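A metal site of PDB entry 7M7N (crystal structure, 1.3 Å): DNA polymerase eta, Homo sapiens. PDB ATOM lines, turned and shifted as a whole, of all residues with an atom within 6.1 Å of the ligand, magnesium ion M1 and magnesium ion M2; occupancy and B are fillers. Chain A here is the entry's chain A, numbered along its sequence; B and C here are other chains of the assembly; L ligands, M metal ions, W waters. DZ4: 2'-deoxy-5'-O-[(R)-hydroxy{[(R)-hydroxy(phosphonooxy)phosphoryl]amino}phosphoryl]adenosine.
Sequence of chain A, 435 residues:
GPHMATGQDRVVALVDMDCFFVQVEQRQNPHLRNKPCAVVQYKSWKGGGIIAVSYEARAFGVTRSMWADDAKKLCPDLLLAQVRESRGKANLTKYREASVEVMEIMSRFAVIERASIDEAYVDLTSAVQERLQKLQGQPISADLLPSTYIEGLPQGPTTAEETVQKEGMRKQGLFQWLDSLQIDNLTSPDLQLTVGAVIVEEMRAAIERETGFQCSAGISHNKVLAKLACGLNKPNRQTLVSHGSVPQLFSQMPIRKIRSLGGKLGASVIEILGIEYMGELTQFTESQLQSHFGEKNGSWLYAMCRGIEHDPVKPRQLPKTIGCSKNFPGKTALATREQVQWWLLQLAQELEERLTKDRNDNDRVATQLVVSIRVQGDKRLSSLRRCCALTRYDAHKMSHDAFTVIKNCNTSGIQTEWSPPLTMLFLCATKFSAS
N6 of AF2 8 of chain B is in hydrogen-bond range of N6 of the ligand, 3.0 Å away.
O2G of the ligand sits at hydrogen-bond distance from OH of Tyr 55, at 2.7 Å.
O4 of DT 4 of chain C lies within hydrogen-bond range of a nitrogen (N6) of the ligand (3.0 Å).
The backbone NH (N) of Cys 19 lies within hydrogen-bond range of an oxygen (O2G) of the ligand, 2.9 Å away.
The guanidinium group (NH1) of Arg 64 is in hydrogen-bond range of a nitrogen (N7) of the ligand (2.9 Å).
The guanidinium group of Arg 58 lies within salt-bridge range of an oxygen (O3G) of the ligand (3.1 Å).
The backbone NH (N) of Phe 20 is in hydrogen-bond range of an oxygen (O2B) of the ligand, at 3.3 Å.
An oxygen (O3') of the ligand is in hydrogen-bond range of the backbone NH (N) of Phe 21 (3.1 Å).
The side-chain amino group (NZ) of Lys 234 is in salt-bridge range of an oxygen (O2G) of the ligand, at 3.1 Å.
Residues that only touch the ligand: Asp 18, Ile 51, DT 5 of chain C, Ala 52 and Ile 117.
Within 4 Å of the ligand: Asp 16, Met 17, Asp 18, Cys 19, Phe 20, Phe 21, Ile 51, Ala 52, Tyr 55, Arg 58, Arg 64, Ile 117, Asp 118, Lys 234, AF2 8 of chain B, DT 4 of chain C and DT 5 of chain C.
The nearest printed residue that does not touch the ligand is Glu 119 (4.3 Å).
Merely in contact with magnesium ion M1: Lys 234.
Magnesium ion M2 is bound by the side-chain carboxylate of Asp 16 (2.1 Å), the side-chain carboxylate of Asp 118 (2.1 Å), water W4 (2.1 Å), the side-chain carboxylate of Glu 119 (2.1 Å), O3' of AF2 8 of chain B (2.1 Å) and an oxygen (O1A) of the ligand (2.2 Å).
Water W4 lies within hydrogen-bond range of an oxygen (O2A) of the ligand, the side-chain amino group (NZ) of Lys 227 and O5' of AF2 8 of chain B.
Water W3 lies within hydrogen-bond range of O2B of the ligand (2.6 Å), N of Val 53 (2.9 Å) and NH2 of Arg 58 (2.9 Å).
Water W8 lies within hydrogen-bond range of O2A of the ligand, OP2 of AF2 8 of chain B and NH1 of Arg 64.
Water W1 lies within hydrogen-bond range of N3 of AF2 8 of chain B and an oxygen (O4') of the ligand.
Water W2 bridges the backbone carbonyl oxygen (O) of Ile 51 (3.0 Å) and a nitrogen (N3A) of the ligand (3.3 Å).
Ser 116 touches magnesium ion M2 (OG to MG, 3.7 Å).
Five residues have an atom within 4 Å of magnesium ion M2: Asp 16, Ser 116, Asp 118, Glu 119 and AF2 8 of chain B.
The nearest printed residue that does not touch magnesium ion M2 is Lys 227 (4.4 Å).
N of Asp 118 lies close to OG of Ser 116 (3.1 Å).
The backbone carbonyl oxygen (O) of Asp 16 sits at hydrogen-bond distance from the side-chain amino group (NZ) of Lys 234, at 3.1 Å.
OE1 of Glu 119 is in salt-bridge range of NZ of Lys 227 (2.8 Å).
The side-chain hydroxyl (OG) of Ser 116 sits close to O3' of AF2 8 of chain B (2.9 Å).
OP1 of AF2 8 of chain B is in salt-bridge range of the side-chain amino group of Lys 227, 3.0 Å away.
The backbone carbonyl oxygen (O) of Met 17 lies close to the side-chain amino group (NZ) of Lys 234 (3.1 Å).
NE of Arg 58 is in hydrogen-bond range of O of Val 53 (2.9 Å).
The side-chain amino group (NZ) of Lys 234 is in salt-bridge range of the side-chain carboxylate (OD1) of Asp 18 (2.9 Å).
Magnesium ion M1 is bound by OD2 of Asp 118 (2.0 Å), OD1 of Asp 16 (2.1 Å), O of Met 17 (2.1 Å), O1G of the ligand (2.2 Å), O1B of the ligand (2.2 Å) and O1A of the ligand (2.3 Å).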
ATOM      1  N   ASP A  16      -3.694  17.955 -16.351  1.00  0.00           N
ATOM      2  CA  ASP A  16      -3.280  18.214 -14.975  1.00  0.00           C
ATOM      3  C   ASP A  16      -2.466  19.494 -14.915  1.00  0.00           C
ATOM      4  O   ASP A  16      -1.464  19.648 -15.633  1.00  0.00           O
ATOM      5  CB  ASP A  16      -2.445  17.063 -14.411  1.00  0.00           C
ATOM      6  CG  ASP A  16      -2.123  17.251 -12.966  1.00  0.00           C
ATOM      7  OD1 ASP A  16      -1.238  18.081 -12.684  1.00  0.00           O
ATOM      8  OD2 ASP A  16      -2.758  16.585 -12.131  1.00  0.00           O
ATOM      9  N   MET A  17      -2.903  20.416 -14.057  1.00  0.00           N
ATOM     10  CA  MET A  17      -2.253  21.720 -13.994  1.00  0.00           C
ATOM     11  C   MET A  17      -0.841  21.618 -13.449  1.00  0.00           C
ATOM     12  O   MET A  17      -0.532  20.800 -12.571  1.00  0.00           O
ATOM     13  CB  MET A  17      -3.076  22.665 -13.101  1.00  0.00           C
ATOM     14  CG  MET A  17      -4.548  22.796 -13.506  1.00  0.00           C
ATOM     15  SD  MET A  17      -4.810  23.266 -15.225  1.00  0.00           S
ATOM     16  CE  MET A  17      -4.062  24.864 -15.226  1.00  0.00           C
ATOM     17  N   ASP A  18       0.061  22.436 -13.993  1.00  0.00           N
ATOM     18  CA  ASP A  18       1.432  22.449 -13.503  1.00  0.00           C
ATOM     19  C   ASP A  18       1.514  23.238 -12.202  1.00  0.00           C
ATOM     20  O   ASP A  18       0.929  24.337 -12.102  1.00  0.00           O
ATOM     21  CB  ASP A  18       2.373  23.045 -14.535  1.00  0.00           C
ATOM     22  CG  ASP A  18       2.432  22.239 -15.825  1.00  0.00           C
ATOM     23  OD1 ASP A  18       2.211  21.014 -15.808  1.00  0.00           O
ATOM     24  OD2 ASP A  18       2.710  22.851 -16.874  1.00  0.00           O
ATOM     25  N   CYS A  19       2.195  22.676 -11.205  1.00  0.00           N
ATOM     26  CA  CYS A  19       2.359  23.284  -9.872  1.00  0.00           C
ATOM     27  C   CYS A  19       1.198  24.206  -9.508  1.00  0.00           C
ATOM     28  O   CYS A  19       1.386  25.410  -9.290  1.00  0.00           O
ATOM     29  CB  CYS A  19       3.732  23.955  -9.721  1.00  0.00           C
ATOM     30  SG  CYS A  19       4.173  25.202 -10.962  1.00  0.00           S
ATOM     31  N   PHE A  20      -0.003  23.642  -9.425  1.00  0.00           N
ATOM     32  CA  PHE A  20      -1.227  24.426  -9.563  1.00  0.00           C
ATOM     33  C   PHE A  20      -1.320  25.573  -8.559  1.00  0.00           C
ATOM     34  O   PHE A  20      -1.522  26.736  -8.960  1.00  0.00           O
ATOM     35  CB  PHE A  20      -2.451  23.525  -9.494  1.00  0.00           C
ATOM     36  CG  PHE A  20      -3.748  24.249  -9.691  1.00  0.00           C
ATOM     37  CD1 PHE A  20      -3.901  25.132 -10.740  1.00  0.00           C
ATOM     38  CD2 PHE A  20      -4.808  24.019  -8.832  1.00  0.00           C
ATOM     39  CE1 PHE A  20      -5.102  25.801 -10.934  1.00  0.00           C
ATOM     40  CE2 PHE A  20      -6.013  24.673  -9.011  1.00  0.00           C
ATOM     41  CZ  PHE A  20      -6.162  25.561 -10.072  1.00  0.00           C
ATOM     42  N   PHE A  21      -1.230  25.293  -7.245  1.00  0.00           N
ATOM     43  CA  PHE A  21      -1.456  26.397  -6.308  1.00  0.00           C
ATOM     44  C   PHE A  21      -0.394  27.474  -6.465  1.00  0.00           C
ATOM     45  O   PHE A  21      -0.675  28.676  -6.264  1.00  0.00           O
ATOM     46  CB  PHE A  21      -1.464  25.932  -4.847  1.00  0.00           C
ATOM     47  CG  PHE A  21      -2.647  25.071  -4.440  1.00  0.00           C
ATOM     48  CD1 PHE A  21      -3.543  24.541  -5.355  1.00  0.00           C
ATOM     49  CD2 PHE A  21      -2.822  24.773  -3.098  1.00  0.00           C
ATOM     50  CE1 PHE A  21      -4.613  23.723  -4.929  1.00  0.00           C
ATOM     51  CE2 PHE A  21      -3.882  23.988  -2.660  1.00  0.00           C
ATOM     52  CZ  PHE A  21      -4.759  23.445  -3.576  1.00  0.00           C
ATOM     53  N   VAL A  22       0.829  27.087  -6.838  1.00  0.00           N
ATOM     54  CA  VAL A  22       1.869  28.080  -7.112  1.00  0.00           C
ATOM     55  C   VAL A  22       1.452  28.993  -8.255  1.00  0.00           C
ATOM     56  O   VAL A  22       1.590  30.215  -8.180  1.00  0.00           O
ATOM     57  CB  VAL A  22       3.220  27.393  -7.375  1.00  0.00           C
ATOM     58  CG1 VAL A  22       4.205  28.387  -7.958  1.00  0.00           C
ATOM     59  CG2 VAL A  22       3.741  26.770  -6.090  1.00  0.00           C
ATOM     60  N   GLN A  41       1.215  26.186   4.227  1.00  0.00           N
ATOM     61  CA  GLN A  41       0.112  26.302   5.170  1.00  0.00           C
ATOM     62  C   GLN A  41       0.695  26.508   6.554  1.00  0.00           C
ATOM     63  O   GLN A  41       1.546  25.728   6.992  1.00  0.00           O
ATOM     64  CB  GLN A  41      -0.763  25.046   5.165  1.00  0.00           C
ATOM     65  CG  GLN A  41      -1.700  24.994   3.994  1.00  0.00           C
ATOM     66  CD  GLN A  41      -2.591  23.768   3.976  1.00  0.00           C
ATOM     67  OE1 GLN A  41      -3.760  23.864   3.631  1.00  0.00           O
ATOM     68  NE2 GLN A  41      -2.038  22.606   4.328  1.00  0.00           N
ATOM     69  N   ILE A  51       2.831  22.668   0.340  1.00  0.00           N
ATOM     70  CA  ILE A  51       1.876  21.848  -0.408  1.00  0.00           C
ATOM     71  C   ILE A  51       2.003  21.978  -1.919  1.00  0.00           C
ATOM     72  O   ILE A  51       1.342  21.200  -2.634  1.00  0.00           O
ATOM     73  CB  ILE A  51       0.413  22.064   0.058  1.00  0.00           C
ATOM     74  CG1 ILE A  51      -0.034  23.519  -0.110  1.00  0.00           C
ATOM     75  CG2 ILE A  51       0.222  21.543   1.491  1.00  0.00           C
ATOM     76  CD1 ILE A  51      -1.514  23.734   0.204  1.00  0.00           C
ATOM     77  N   ALA A  52       2.815  22.899  -2.439  1.00  0.00           N
ATOM     78  CA  ALA A  52       3.029  23.005  -3.884  1.00  0.00           C
ATOM     79  C   ALA A  52       4.338  23.740  -4.118  1.00  0.00           C
ATOM     80  O   ALA A  52       4.716  24.618  -3.342  1.00  0.00           O
ATOM     81  CB  ALA A  52       1.871  23.757  -4.565  1.00  0.00           C
ATOM     82  N   VAL A  53       5.034  23.375  -5.211  1.00  0.00           N
ATOM     83  CA  VAL A  53       6.412  23.795  -5.448  1.00  0.00           C
ATOM     84  C   VAL A  53       6.589  24.104  -6.933  1.00  0.00           C
ATOM     85  O   VAL A  53       6.281  23.268  -7.783  1.00  0.00           O
ATOM     86  CB  VAL A  53       7.429  22.700  -5.037  1.00  0.00           C
ATOM     87  CG1 VAL A  53       8.846  23.203  -5.187  1.00  0.00           C
ATOM     88  CG2 VAL A  53       7.159  22.196  -3.616  1.00  0.00           C
ATOM     89  N   TYR A  55       8.575  24.647 -10.487  1.00  0.00           N
ATOM     90  CA  TYR A  55       9.621  23.817 -11.095  1.00  0.00           C
ATOM     91  C   TYR A  55      11.015  24.379 -10.841  1.00  0.00           C
ATOM     92  O   TYR A  55      11.975  23.604 -10.619  1.00  0.00           O
ATOM     93  CB  TYR A  55       9.291  23.559 -12.573  1.00  0.00           C
ATOM     94  CG  TYR A  55       8.234  22.501 -12.709  1.00  0.00           C
ATOM     95  CD1 TYR A  55       6.883  22.795 -12.534  1.00  0.00           C
ATOM     96  CD2 TYR A  55       8.583  21.177 -12.933  1.00  0.00           C
ATOM     97  CE1 TYR A  55       5.921  21.814 -12.612  1.00  0.00           C
ATOM     98  CE2 TYR A  55       7.635  20.190 -13.027  1.00  0.00           C
ATOM     99  CZ  TYR A  55       6.296  20.502 -12.856  1.00  0.00           C
ATOM    100  OH  TYR A  55       5.354  19.507 -12.936  1.00  0.00           O
ATOM    101  N   ARG A  58      11.844  23.081  -7.508  1.00  0.00           N
ATOM    102  CA  ARG A  58      12.111  21.645  -7.541  1.00  0.00           C
ATOM    103  C   ARG A  58      13.540  21.361  -7.971  1.00  0.00           C
ATOM    104  O   ARG A  58      14.128  20.364  -7.537  1.00  0.00           O
ATOM    105  CB  ARG A  58      11.139  20.915  -8.460  1.00  0.00           C
ATOM    106  CG  ARG A  58       9.680  21.064  -8.078  1.00  0.00           C
ATOM    107  CD  ARG A  58       8.752  20.266  -8.988  1.00  0.00           C
ATOM    108  NE  ARG A  58       7.372  20.733  -8.810  1.00  0.00           N
ATOM    109  CZ  ARG A  58       6.288  20.119  -9.275  1.00  0.00           C
ATOM    110  NH1 ARG A  58       6.381  18.984  -9.951  1.00  0.00           N
ATOM    111  NH2 ARG A  58       5.089  20.658  -9.052  1.00  0.00           N
ATOM    112  N   ARG A  64       7.038  18.861  -1.847  1.00  0.00           N
ATOM    113  CA  ARG A  64       5.846  18.853  -1.010  1.00  0.00           C
ATOM    114  C   ARG A  64       6.160  18.117   0.291  1.00  0.00           C
ATOM    115  O   ARG A  64       7.006  17.223   0.337  1.00  0.00           O
ATOM    116  CB  ARG A  64       4.732  18.120  -1.753  1.00  0.00           C
ATOM    117  CG  ARG A  64       3.391  18.029  -1.057  1.00  0.00           C
ATOM    118  CD  ARG A  64       2.365  17.388  -1.983  1.00  0.00           C
ATOM    119  NE  ARG A  64       2.400  15.932  -1.948  1.00  0.00           N
ATOM    120  CZ  ARG A  64       1.906  15.153  -2.908  1.00  0.00           C
ATOM    121  NH1 ARG A  64       1.354  15.693  -3.989  1.00  0.00           N
ATOM    122  NH2 ARG A  64       1.974  13.832  -2.792  1.00  0.00           N
ATOM    123  N   SER A 116      -9.409  15.694  -9.573  1.00  0.00           N
ATOM    124  CA  SER A 116      -8.869  16.350  -8.395  1.00  0.00           C
ATOM    125  C   SER A 116      -9.062  17.835  -8.587  1.00  0.00           C
ATOM    126  O   SER A 116      -9.525  18.288  -9.635  1.00  0.00           O
ATOM    127  CB  SER A 116      -7.382  16.028  -8.171  1.00  0.00           C
ATOM    128  OG  SER A 116      -6.527  16.903  -8.902  1.00  0.00           O
ATOM    129  N   ILE A 117      -8.641  18.607  -7.577  1.00  0.00           N
ATOM    130  CA  ILE A 117      -8.722  20.059  -7.683  1.00  0.00           C
ATOM    131  C   ILE A 117      -8.026  20.585  -8.932  1.00  0.00           C
ATOM    132  O   ILE A 117      -8.368  21.665  -9.430  1.00  0.00           O
ATOM    133  CB  ILE A 117      -8.205  20.730  -6.397  1.00  0.00           C
ATOM    134  CG1 ILE A 117      -8.694  22.186  -6.328  1.00  0.00           C
ATOM    135  CG2 ILE A 117      -6.678  20.619  -6.329  1.00  0.00           C
ATOM    136  CD1 ILE A 117      -8.494  22.829  -4.967  1.00  0.00           C
ATOM    137  N   ASP A 118      -7.038  19.856  -9.477  1.00  0.00           N
ATOM    138  CA  ASP A 118      -6.284  20.395 -10.612  1.00  0.00           C
ATOM    139  C   ASP A 118      -6.284  19.477 -11.814  1.00  0.00           C
ATOM    140  O   ASP A 118      -5.430  19.646 -12.694  1.00  0.00           O
ATOM    141  CB  ASP A 118      -4.862  20.795 -10.215  1.00  0.00           C
ATOM    142  CG  ASP A 118      -3.842  19.684 -10.429  1.00  0.00           C
ATOM    143  OD1 ASP A 118      -4.160  18.498 -10.144  1.00  0.00           O
ATOM    144  OD2 ASP A 118      -2.729  20.025 -10.886  1.00  0.00           O
ATOM    145  N   GLU A 119      -7.195  18.502 -11.884  1.00  0.00           N
ATOM    146  CA  GLU A 119      -7.103  17.640 -13.064  1.00  0.00           C
ATOM    147  C   GLU A 119      -8.449  17.046 -13.405  1.00  0.00           C
ATOM    148  O   GLU A 119      -9.290  16.803 -12.520  1.00  0.00           O
ATOM    149  CB  GLU A 119      -6.073  16.520 -12.910  1.00  0.00           C
ATOM    150  CG  GLU A 119      -6.473  15.392 -11.997  1.00  0.00           C
ATOM    151  CD  GLU A 119      -5.261  14.810 -11.317  1.00  0.00           C
ATOM    152  OE1 GLU A 119      -4.836  13.689 -11.676  1.00  0.00           O
ATOM    153  OE2 GLU A 119      -4.705  15.495 -10.434  1.00  0.00           O
ATOM    154  N   LYS A 227      -3.257   9.260 -17.619  1.00  0.00           N
ATOM    155  CA  LYS A 227      -2.637   9.806 -16.422  1.00  0.00           C
ATOM    156  C   LYS A 227      -1.126   9.562 -16.422  1.00  0.00           C
ATOM    157  O   LYS A 227      -0.337  10.478 -16.143  1.00  0.00           O
ATOM    158  CB  LYS A 227      -3.288   9.201 -15.171  1.00  0.00           C
ATOM    159  CG  LYS A 227      -2.616   9.600 -13.843  1.00  0.00           C
ATOM    160  CD  LYS A 227      -2.711  11.110 -13.543  1.00  0.00           C
ATOM    161  CE  LYS A 227      -2.222  11.369 -12.131  1.00  0.00           C
ATOM    162  NZ  LYS A 227      -2.205  12.812 -11.755  1.00  0.00           N
ATOM    163  N   LYS A 234       5.836  16.564 -18.138  1.00  0.00           N
ATOM    164  CA  LYS A 234       5.594  17.780 -17.367  1.00  0.00           C
ATOM    165  C   LYS A 234       6.906  18.542 -17.183  1.00  0.00           C
ATOM    166  O   LYS A 234       7.955  17.927 -16.983  1.00  0.00           O
ATOM    167  CB  LYS A 234       5.075  17.406 -15.982  1.00  0.00           C
ATOM    168  CG  LYS A 234       3.601  17.580 -15.847  1.00  0.00           C
ATOM    169  CD  LYS A 234       3.105  17.233 -14.466  1.00  0.00           C
ATOM    170  CE  LYS A 234       1.598  17.418 -14.415  1.00  0.00           C
ATOM    171  NZ  LYS A 234       1.203  18.844 -14.222  1.00  0.00           N
ATOM    172  N   PRO A 235       6.872  19.886 -17.170  1.00  0.00           N
ATOM    173  CA  PRO A 235       5.667  20.728 -17.281  1.00  0.00           C
ATOM    174  C   PRO A 235       5.434  21.262 -18.694  1.00  0.00           C
ATOM    175  O   PRO A 235       6.317  21.191 -19.555  1.00  0.00           O
ATOM    176  CB  PRO A 235       6.005  21.895 -16.360  1.00  0.00           C
ATOM    177  CG  PRO A 235       7.485  22.065 -16.540  1.00  0.00           C
ATOM    178  CD  PRO A 235       8.052  20.680 -16.798  1.00  0.00           C
ATOM    179  P    DA B   7      -1.835   5.478  -5.408  1.00  0.00           P
ATOM    180  OP1  DA B   7      -1.585   4.895  -6.742  1.00  0.00           O
ATOM    181  OP2  DA B   7      -0.791   5.430  -4.386  1.00  0.00           O
ATOM    182  O5'  DA B   7      -2.226   7.025  -5.520  1.00  0.00           O
ATOM    183  C5'  DA B   7      -3.298   7.422  -6.295  1.00  0.00           C
ATOM    184  C4'  DA B   7      -3.643   8.861  -6.000  1.00  0.00           C
ATOM    185  O4'  DA B   7      -4.177   8.981  -4.659  1.00  0.00           O
ATOM    186  C3'  DA B   7      -2.456   9.843  -6.060  1.00  0.00           C
ATOM    187  O3'  DA B   7      -2.699  10.735  -7.119  1.00  0.00           O
ATOM    188  C2'  DA B   7      -2.485  10.546  -4.710  1.00  0.00           C
ATOM    189  C1'  DA B   7      -3.908  10.258  -4.224  1.00  0.00           C
ATOM    190  N9   DA B   7      -4.039  10.299  -2.778  1.00  0.00           N
ATOM    191  C8   DA B   7      -3.374   9.535  -1.869  1.00  0.00           C
ATOM    192  N7   DA B   7      -3.666   9.823  -0.630  1.00  0.00           N
ATOM    193  C5   DA B   7      -4.580  10.866  -0.737  1.00  0.00           C
ATOM    194  C6   DA B   7      -5.267  11.621   0.221  1.00  0.00           C
ATOM    195  N6   DA B   7      -5.131  11.442   1.544  1.00  0.00           N
ATOM    196  N1   DA B   7      -6.092  12.597  -0.220  1.00  0.00           N
ATOM    197  C2   DA B   7      -6.226  12.786  -1.546  1.00  0.00           C
ATOM    198  N3   DA B   7      -5.635  12.127  -2.544  1.00  0.00           N
ATOM    199  C4   DA B   7      -4.809  11.176  -2.056  1.00  0.00           C
ATOM    200  F   AF2 B   8      -5.099  17.176  -6.018  1.00  0.00           F
ATOM    201  P   AF2 B   8      -1.634  11.806  -7.616  1.00  0.00           P
ATOM    202  N1  AF2 B   8      -4.032  15.952   0.169  1.00  0.00           N
ATOM    203  C2  AF2 B   8      -4.741  16.587  -0.772  1.00  0.00           C
ATOM    204  N3  AF2 B   8      -4.787  16.370  -2.078  1.00  0.00           N
ATOM    205  C4  AF2 B   8      -3.980  15.348  -2.416  1.00  0.00           C
ATOM    206  C5  AF2 B   8      -3.175  14.608  -1.573  1.00  0.00           C
ATOM    207  C6  AF2 B   8      -3.227  14.932  -0.202  1.00  0.00           C
ATOM    208  N6  AF2 B   8      -2.516  14.307   0.736  1.00  0.00           N
ATOM    209  N7  AF2 B   8      -2.467  13.640  -2.278  1.00  0.00           N
ATOM    210  C8  AF2 B   8      -2.848  13.827  -3.512  1.00  0.00           C
ATOM    211  N9  AF2 B   8      -3.726  14.868  -3.686  1.00  0.00           N
ATOM    212  C1' AF2 B   8      -4.459  15.240  -4.889  1.00  0.00           C
ATOM    213  OP2 AF2 B   8      -0.411  11.815  -6.781  1.00  0.00           O
ATOM    214  C2' AF2 B   8      -3.981  16.435  -5.711  1.00  0.00           C
ATOM    215  OP1 AF2 B   8      -1.510  11.636  -9.075  1.00  0.00           O
ATOM    216  C3' AF2 B   8      -3.500  15.781  -6.999  1.00  0.00           C
ATOM    217  O3' AF2 B   8      -3.745  16.627  -8.108  1.00  0.00           O
ATOM    218  C4' AF2 B   8      -4.353  14.524  -7.107  1.00  0.00           C
ATOM    219  O4' AF2 B   8      -4.503  14.106  -5.731  1.00  0.00           O
ATOM    220  C5' AF2 B   8      -3.712  13.408  -7.884  1.00  0.00           C
ATOM    221  O5' AF2 B   8      -2.390  13.179  -7.348  1.00  0.00           O
ATOM    222  P    DT C   4       0.540  17.267   9.969  1.00  0.00           P
ATOM    223  OP1  DT C   4       0.302  17.669  11.375  1.00  0.00           O
ATOM    224  OP2  DT C   4       0.234  15.909   9.489  1.00  0.00           O
ATOM    225  O5'  DT C   4      -0.312  18.266   9.056  1.00  0.00           O
ATOM    226  C5'  DT C   4      -0.178  19.660   9.213  1.00  0.00           C
ATOM    227  C4'  DT C   4      -1.210  20.377   8.365  1.00  0.00           C
ATOM    228  O4'  DT C   4      -1.009  20.047   6.971  1.00  0.00           O
ATOM    229  C3'  DT C   4      -2.661  20.033   8.681  1.00  0.00           C
ATOM    230  O3'  DT C   4      -3.442  21.175   8.472  1.00  0.00           O
ATOM    231  C2'  DT C   4      -2.971  18.937   7.657  1.00  0.00           C
ATOM    232  C1'  DT C   4      -2.167  19.408   6.457  1.00  0.00           C
ATOM    233  N1   DT C   4      -1.722  18.346   5.517  1.00  0.00           N
ATOM    234  C2   DT C   4      -1.879  18.585   4.171  1.00  0.00           C
ATOM    235  O2   DT C   4      -2.408  19.586   3.747  1.00  0.00           O
ATOM    236  N3   DT C   4      -1.426  17.600   3.357  1.00  0.00           N
ATOM    237  C4   DT C   4      -0.807  16.422   3.727  1.00  0.00           C
ATOM    238  O4   DT C   4      -0.428  15.599   2.890  1.00  0.00           O
ATOM    239  C5   DT C   4      -0.654  16.229   5.154  1.00  0.00           C
ATOM    240  C7   DT C   4      -0.005  14.980   5.691  1.00  0.00           C
ATOM    241  C6   DT C   4      -1.099  17.203   5.973  1.00  0.00           C
ATOM    242  P    DT C   5      -5.014  21.166   8.797  1.00  0.00           P
ATOM    243  OP1  DT C   5      -5.313  22.497   9.360  1.00  0.00           O
ATOM    244  OP2  DT C   5      -5.398  19.950   9.559  1.00  0.00           O
ATOM    245  O5'  DT C   5      -5.677  21.043   7.339  1.00  0.00           O
ATOM    246  C5'  DT C   5      -5.543  22.095   6.399  1.00  0.00           C
ATOM    247  C4'  DT C   5      -6.274  21.753   5.126  1.00  0.00           C
ATOM    248  O4'  DT C   5      -5.572  20.670   4.456  1.00  0.00           O
ATOM    249  C3'  DT C   5      -7.710  21.244   5.317  1.00  0.00           C
ATOM    250  O3'  DT C   5      -8.529  21.769   4.273  1.00  0.00           O
ATOM    251  C2'  DT C   5      -7.545  19.726   5.204  1.00  0.00           C
ATOM    252  C1'  DT C   5      -6.497  19.670   4.114  1.00  0.00           C
ATOM    253  N1   DT C   5      -5.768  18.387   3.995  1.00  0.00           N
ATOM    254  C2   DT C   5      -5.369  17.988   2.748  1.00  0.00           C
ATOM    255  O2   DT C   5      -5.603  18.632   1.748  1.00  0.00           O
ATOM    256  N3   DT C   5      -4.693  16.800   2.716  1.00  0.00           N
ATOM    257  C4   DT C   5      -4.364  15.994   3.785  1.00  0.00           C
ATOM    258  O4   DT C   5      -3.746  14.941   3.645  1.00  0.00           O
ATOM    259  C5   DT C   5      -4.797  16.473   5.074  1.00  0.00           C
ATOM    260  C7   DT C   5      -4.505  15.680   6.315  1.00  0.00           C
ATOM    261  C6   DT C   5      -5.468  17.644   5.124  1.00  0.00           C
HETATM  262  N1  DZ4 L   1      -1.692  18.106   0.644  1.00  0.00           N
HETATM  263  C2  DZ4 L   1      -2.374  19.205   0.298  1.00  0.00           C
HETATM  264  N3  DZ4 L   1      -2.559  19.739  -0.913  1.00  0.00           N
HETATM  265  C4  DZ4 L   1      -1.958  18.992  -1.849  1.00  0.00           C
HETATM  266  C5  DZ4 L   1      -1.235  17.842  -1.660  1.00  0.00           C
HETATM  267  C6  DZ4 L   1      -1.100  17.390  -0.335  1.00  0.00           C
HETATM  268  N6  DZ4 L   1      -0.417  16.286  -0.041  1.00  0.00           N
HETATM  269  N7  DZ4 L   1      -0.767  17.358  -2.876  1.00  0.00           N
HETATM  270  C8  DZ4 L   1      -1.205  18.213  -3.759  1.00  0.00           C
HETATM  271  N9  DZ4 L   1      -1.939  19.225  -3.202  1.00  0.00           N
HETATM  272  PA  DZ4 L   1      -0.706  17.855  -8.054  1.00  0.00           P
HETATM  273  PB  DZ4 L   1       1.006  20.166  -8.638  1.00  0.00           P
HETATM  274  PG  DZ4 L   1       2.503  19.038 -10.879  1.00  0.00           P
HETATM  275  C1' DZ4 L   1      -2.583  20.357  -3.850  1.00  0.00           C
HETATM  276  O1A DZ4 L   1      -1.330  17.865  -9.365  1.00  0.00           O
HETATM  277  O1B DZ4 L   1      -0.046  20.645  -9.521  1.00  0.00           O
HETATM  278  O1G DZ4 L   1       1.149  18.469 -11.176  1.00  0.00           O
HETATM  279  C2' DZ4 L   1      -1.595  21.455  -4.221  1.00  0.00           C
HETATM  280  O2A DZ4 L   1      -0.560  16.395  -7.548  1.00  0.00           O
HETATM  281  O2B DZ4 L   1       1.368  21.245  -7.577  1.00  0.00           O
HETATM  282  O2G DZ4 L   1       2.952  20.015 -11.925  1.00  0.00           O
HETATM  283  C3' DZ4 L   1      -1.302  21.184  -5.689  1.00  0.00           C
HETATM  284  O3' DZ4 L   1      -0.953  22.369  -6.395  1.00  0.00           O
HETATM  285  N3A DZ4 L   1       0.687  18.701  -7.976  1.00  0.00           N
HETATM  286  O3B DZ4 L   1       2.313  19.899  -9.535  1.00  0.00           O
HETATM  287  O3G DZ4 L   1       3.528  17.981 -10.585  1.00  0.00           O
HETATM  288  C4' DZ4 L   1      -2.633  20.629  -6.179  1.00  0.00           C
HETATM  289  O4' DZ4 L   1      -3.181  19.908  -5.063  1.00  0.00           O
HETATM  290  C5' DZ4 L   1      -2.518  19.692  -7.352  1.00  0.00           C
HETATM  291  O5' DZ4 L   1      -1.689  18.558  -6.987  1.00  0.00           O
HETATM  292 MG    MG M   1      -0.832  19.313 -11.076  1.00  0.00          MG
HETATM  293 MG    MG M   2      -3.037  16.764 -10.106  1.00  0.00          MG
HETATM  294  O   HOH W   1      -5.619  18.717  -3.548  1.00  0.00           O
HETATM  295  O   HOH W   2       1.868  19.277  -4.895  1.00  0.00           O
HETATM  296  O   HOH W   3       3.765  21.135  -6.474  1.00  0.00           O
HETATM  297  O   HOH W   4      -1.728  15.140  -9.854  1.00  0.00           O
HETATM  298  O   HOH W   5      -4.810  21.509  -0.618  1.00  0.00           O
HETATM  299  O   HOH W   6       0.538  15.820 -11.325  1.00  0.00           O
HETATM  300  O   HOH W   7       3.432  17.173  -7.964  1.00  0.00           O
HETATM  301  O   HOH W   8       1.016  14.287  -6.949  1.00  0.00           O
